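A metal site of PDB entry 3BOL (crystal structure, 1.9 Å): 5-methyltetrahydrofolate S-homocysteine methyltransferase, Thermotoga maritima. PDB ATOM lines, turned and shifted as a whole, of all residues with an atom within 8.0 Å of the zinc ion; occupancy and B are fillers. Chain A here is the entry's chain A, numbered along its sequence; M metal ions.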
ATOM      1  N   ALA A  21       5.946 -16.480  13.835  1.00  0.00           N
ATOM      2  CA  ALA A  21       4.784 -15.738  14.393  1.00  0.00           C
ATOM      3  C   ALA A  21       3.457 -16.439  14.164  1.00  0.00           C
ATOM      4  O   ALA A  21       3.311 -17.227  13.223  1.00  0.00           O
ATOM      5  CB  ALA A  21       4.726 -14.303  13.813  1.00  0.00           C
ATOM      6  N   GLU A 146       7.284 -14.778  27.272  1.00  0.00           N
ATOM      7  CA  GLU A 146       7.727 -13.987  26.130  1.00  0.00           C
ATOM      8  C   GLU A 146       7.419 -12.528  26.282  1.00  0.00           C
ATOM      9  O   GLU A 146       6.386 -12.218  26.831  1.00  0.00           O
ATOM     10  CB  GLU A 146       6.997 -14.434  24.875  1.00  0.00           C
ATOM     11  CG  GLU A 146       7.708 -15.531  24.094  1.00  0.00           C
ATOM     12  CD  GLU A 146       7.053 -15.748  22.756  1.00  0.00           C
ATOM     13  OE1 GLU A 146       5.813 -15.886  22.697  1.00  0.00           O
ATOM     14  OE2 GLU A 146       7.783 -15.812  21.764  1.00  0.00           O
ATOM     15  N   THR A 147       8.329 -11.657  25.803  1.00  0.00           N
ATOM     16  CA  THR A 147       8.001 -10.237  25.579  1.00  0.00           C
ATOM     17  C   THR A 147       7.704  -9.486  26.860  1.00  0.00           C
ATOM     18  O   THR A 147       6.905  -8.494  26.853  1.00  0.00           O
ATOM     19  CB  THR A 147       6.798 -10.054  24.641  1.00  0.00           C
ATOM     20  OG1 THR A 147       6.679 -11.173  23.738  1.00  0.00           O
ATOM     21  CG2 THR A 147       6.857  -8.675  23.882  1.00  0.00           C
ATOM     22  N   THR A 175      11.907  -7.796  26.534  1.00  0.00           N
ATOM     23  CA  THR A 175      11.988  -7.158  25.203  1.00  0.00           C
ATOM     24  C   THR A 175      12.573  -5.790  25.483  1.00  0.00           C
ATOM     25  O   THR A 175      12.205  -5.117  26.494  1.00  0.00           O
ATOM     26  CB  THR A 175      10.662  -7.155  24.397  1.00  0.00           C
ATOM     27  OG1 THR A 175      10.914  -6.755  23.037  1.00  0.00           O
ATOM     28  CG2 THR A 175       9.604  -6.236  25.021  1.00  0.00           C
ATOM     29  N   ASN A 206      13.011 -11.402  22.911  1.00  0.00           N
ATOM     30  CA  ASN A 206      12.226 -11.498  21.689  1.00  0.00           C
ATOM     31  C   ASN A 206      11.538 -10.169  21.419  1.00  0.00           C
ATOM     32  O   ASN A 206      11.366  -9.372  22.362  1.00  0.00           O
ATOM     33  CB  ASN A 206      11.198 -12.652  21.697  1.00  0.00           C
ATOM     34  CG  ASN A 206      10.013 -12.395  22.615  1.00  0.00           C
ATOM     35  OD1 ASN A 206      10.143 -12.480  23.825  1.00  0.00           O
ATOM     36  ND2 ASN A 206       8.877 -12.001  22.027  1.00  0.00           N
ATOM     37  N   CYS A 207      11.149  -9.975  20.153  1.00  0.00           N
ATOM     38  CA  CYS A 207      10.333  -8.798  19.764  1.00  0.00           C
ATOM     39  C   CYS A 207      11.056  -7.463  19.849  1.00  0.00           C
ATOM     40  O   CYS A 207      12.222  -7.375  20.189  1.00  0.00           O
ATOM     41  CB  CYS A 207       9.030  -8.701  20.612  1.00  0.00           C
ATOM     42  SG  CYS A 207       7.547  -7.972  19.725  1.00  0.00           S
ATOM     43  N   SER A 208      10.310  -6.392  19.549  1.00  0.00           N
ATOM     44  CA  SER A 208      10.764  -4.986  19.587  1.00  0.00           C
ATOM     45  C   SER A 208      11.718  -4.593  18.465  1.00  0.00           C
ATOM     46  O   SER A 208      11.634  -3.458  17.935  1.00  0.00           O
ATOM     47  CB  SER A 208      11.377  -4.576  20.932  1.00  0.00           C
ATOM     48  OG  SER A 208      10.347  -4.388  21.884  1.00  0.00           O
ATOM     49  N   LEU A 209      12.639  -5.504  18.143  1.00  0.00           N
ATOM     50  CA  LEU A 209      13.786  -5.232  17.224  1.00  0.00           C
ATOM     51  C   LEU A 209      14.007  -6.409  16.273  1.00  0.00           C
ATOM     52  O   LEU A 209      13.508  -7.518  16.532  1.00  0.00           O
ATOM     53  CB  LEU A 209      15.071  -4.900  17.984  1.00  0.00           C
ATOM     54  CG  LEU A 209      14.995  -3.737  18.985  1.00  0.00           C
ATOM     55  CD1 LEU A 209      16.223  -3.770  19.830  1.00  0.00           C
ATOM     56  CD2 LEU A 209      14.870  -2.417  18.209  1.00  0.00           C
ATOM     57  N   GLU A 232      14.336 -14.593  19.667  1.00  0.00           N
ATOM     58  CA  GLU A 232      13.361 -14.574  18.626  1.00  0.00           C
ATOM     59  C   GLU A 232      13.208 -13.125  18.160  1.00  0.00           C
ATOM     60  O   GLU A 232      12.356 -12.377  18.691  1.00  0.00           O
ATOM     61  CB  GLU A 232      11.977 -15.052  19.113  1.00  0.00           C
ATOM     62  CG  GLU A 232      11.950 -16.478  19.690  1.00  0.00           C
ATOM     63  CD  GLU A 232      10.619 -16.719  20.337  1.00  0.00           C
ATOM     64  OE1 GLU A 232       9.802 -17.427  19.741  1.00  0.00           O
ATOM     65  OE2 GLU A 232      10.361 -16.091  21.360  1.00  0.00           O
ATOM     66  N   PRO A 233      14.050 -12.709  17.208  1.00  0.00           N
ATOM     67  CA  PRO A 233      13.875 -11.345  16.657  1.00  0.00           C
ATOM     68  C   PRO A 233      12.608 -11.184  15.820  1.00  0.00           C
ATOM     69  O   PRO A 233      12.062 -12.142  15.282  1.00  0.00           O
ATOM     70  CB  PRO A 233      15.136 -11.148  15.803  1.00  0.00           C
ATOM     71  CG  PRO A 233      16.097 -12.277  16.260  1.00  0.00           C
ATOM     72  CD  PRO A 233      15.221 -13.409  16.630  1.00  0.00           C
ATOM     73  N   ASN A 234      12.085  -9.956  15.741  1.00  0.00           N
ATOM     74  CA  ASN A 234      11.097  -9.685  14.732  1.00  0.00           C
ATOM     75  C   ASN A 234      11.818  -9.755  13.374  1.00  0.00           C
ATOM     76  O   ASN A 234      13.017  -9.616  13.289  1.00  0.00           O
ATOM     77  CB  ASN A 234      10.587  -8.250  14.879  1.00  0.00           C
ATOM     78  CG  ASN A 234       9.668  -8.056  16.055  1.00  0.00           C
ATOM     79  OD1 ASN A 234       9.139  -9.026  16.587  1.00  0.00           O
ATOM     80  ND2 ASN A 234       9.429  -6.780  16.432  1.00  0.00           N
ATOM     81  N   ALA A 235      11.058  -9.986  12.330  1.00  0.00           N
ATOM     82  CA  ALA A 235      11.564  -9.980  10.966  1.00  0.00           C
ATOM     83  C   ALA A 235      11.883  -8.527  10.525  1.00  0.00           C
ATOM     84  O   ALA A 235      11.169  -7.950   9.714  1.00  0.00           O
ATOM     85  CB  ALA A 235      10.562 -10.647  10.060  1.00  0.00           C
ATOM     86  N   GLY A 236      12.953  -7.981  11.078  1.00  0.00           N
ATOM     87  CA  GLY A 236      13.457  -6.638  10.751  1.00  0.00           C
ATOM     88  C   GLY A 236      12.700  -5.515  11.458  1.00  0.00           C
ATOM     89  O   GLY A 236      11.817  -5.777  12.301  1.00  0.00           O
ATOM     90  N   TYR A 247       6.493  -6.309   8.942  1.00  0.00           N
ATOM     91  CA  TYR A 247       7.853  -6.693   9.311  1.00  0.00           C
ATOM     92  C   TYR A 247       8.459  -7.407   8.106  1.00  0.00           C
ATOM     93  O   TYR A 247       8.252  -8.592   7.930  1.00  0.00           O
ATOM     94  CB  TYR A 247       7.849  -7.558  10.583  1.00  0.00           C
ATOM     95  CG  TYR A 247       7.480  -6.774  11.825  1.00  0.00           C
ATOM     96  CD1 TYR A 247       8.420  -6.008  12.482  1.00  0.00           C
ATOM     97  CD2 TYR A 247       6.154  -6.762  12.305  1.00  0.00           C
ATOM     98  CE1 TYR A 247       8.081  -5.251  13.600  1.00  0.00           C
ATOM     99  CE2 TYR A 247       5.808  -6.014  13.432  1.00  0.00           C
ATOM    100  CZ  TYR A 247       6.766  -5.264  14.062  1.00  0.00           C
ATOM    101  OH  TYR A 247       6.447  -4.515  15.176  1.00  0.00           O
ATOM    102  N   GLY A 271      11.753 -17.076  15.489  1.00  0.00           N
ATOM    103  CA  GLY A 271      11.365 -15.709  15.108  1.00  0.00           C
ATOM    104  C   GLY A 271      10.088 -15.189  15.786  1.00  0.00           C
ATOM    105  O   GLY A 271       9.233 -15.965  16.248  1.00  0.00           O
ATOM    106  N   CYS A 272       9.943 -13.855  15.798  1.00  0.00           N
ATOM    107  CA  CYS A 272       8.773 -13.238  16.382  1.00  0.00           C
ATOM    108  C   CYS A 272       7.980 -12.599  15.229  1.00  0.00           C
ATOM    109  O   CYS A 272       8.011 -13.062  14.070  1.00  0.00           O
ATOM    110  CB  CYS A 272       9.281 -12.169  17.373  1.00  0.00           C
ATOM    111  SG  CYS A 272       8.058 -11.548  18.609  1.00  0.00           S
ATOM    112  N   CYS A 273       7.292 -11.503  15.518  1.00  0.00           N
ATOM    113  CA  CYS A 273       6.474 -10.806  14.529  1.00  0.00           C
ATOM    114  C   CYS A 273       7.068 -10.824  13.141  1.00  0.00           C
ATOM    115  O   CYS A 273       8.181 -10.411  12.954  1.00  0.00           O
ATOM    116  CB  CYS A 273       6.307  -9.330  14.907  1.00  0.00           C
ATOM    117  SG  CYS A 273       5.728  -9.059  16.597  1.00  0.00           S
ATOM    118  N   GLY A 274       6.278 -11.262  12.185  1.00  0.00           N
ATOM    119  CA  GLY A 274       6.629 -11.103  10.781  1.00  0.00           C
ATOM    120  C   GLY A 274       7.329 -12.339  10.253  1.00  0.00           C
ATOM    121  O   GLY A 274       7.491 -12.517   9.033  1.00  0.00           O
ATOM    122  N   THR A 275       7.719 -13.247  11.174  1.00  0.00           N
ATOM    123  CA  THR A 275       8.394 -14.499  10.789  1.00  0.00           C
ATOM    124  C   THR A 275       7.344 -15.504  10.309  1.00  0.00           C
ATOM    125  O   THR A 275       6.268 -15.658  10.945  1.00  0.00           O
ATOM    126  CB  THR A 275       9.171 -15.124  11.979  1.00  0.00           C
ATOM    127  OG1 THR A 275      10.058 -14.171  12.516  1.00  0.00           O
ATOM    128  CG2 THR A 275      10.055 -16.348  11.526  1.00  0.00           C
HETATM  129 ZN    ZN M   1       7.550  -9.331  17.961  1.00  0.00          ZN
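The side-chain amide nitrogen (ND2) of Asn 234 sits close to the backbone NH (N) of Ser 208 (3.3 Å). N of Asn 234 is in hydrogen-bond range of O of Leu 209 (2.9 Å). The backbone carbonyl oxygen of Glu 232 sits at hydrogen-bond distance from the backbone NH of Cys 207, at 3.1 Å. O of Cys 207 sits at hydrogen-bond distance from OG1 of Thr 175 (3.2 Å). The backbone NH of Ala 235 lies within hydrogen-bond range of the backbone carbonyl oxygen of Cys 273, 3.0 Å away. ND2 of Asn 206 sits close to SG of Cys 272 (3.5 Å). The backbone NH (N) of Cys 272 lies within hydrogen-bond range of the backbone carbonyl oxygen (O) of Pro 233, at 2.8 Å. OG1 of Thr 275 is in hydrogen-bond range of O of Cys 272, at 2.8 Å.
Four residues have an atom within 4 Å of the zinc ion: Cys 207, Asn 234, Cys 272 and Cys 273. Along chain A the residues within 4 Å of the zinc ion span positions 207 to 273.
The zinc ion is bound by the side-chain amide oxygen (OD1) of Asn 234 (2.1 Å), the side-chain sulfur (SG) of Cys 207 (2.2 Å), the side-chain sulfur (SG) of Cys 273 (2.3 Å) and the side-chain sulfur (SG) of Cys 272 (2.4 Å).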
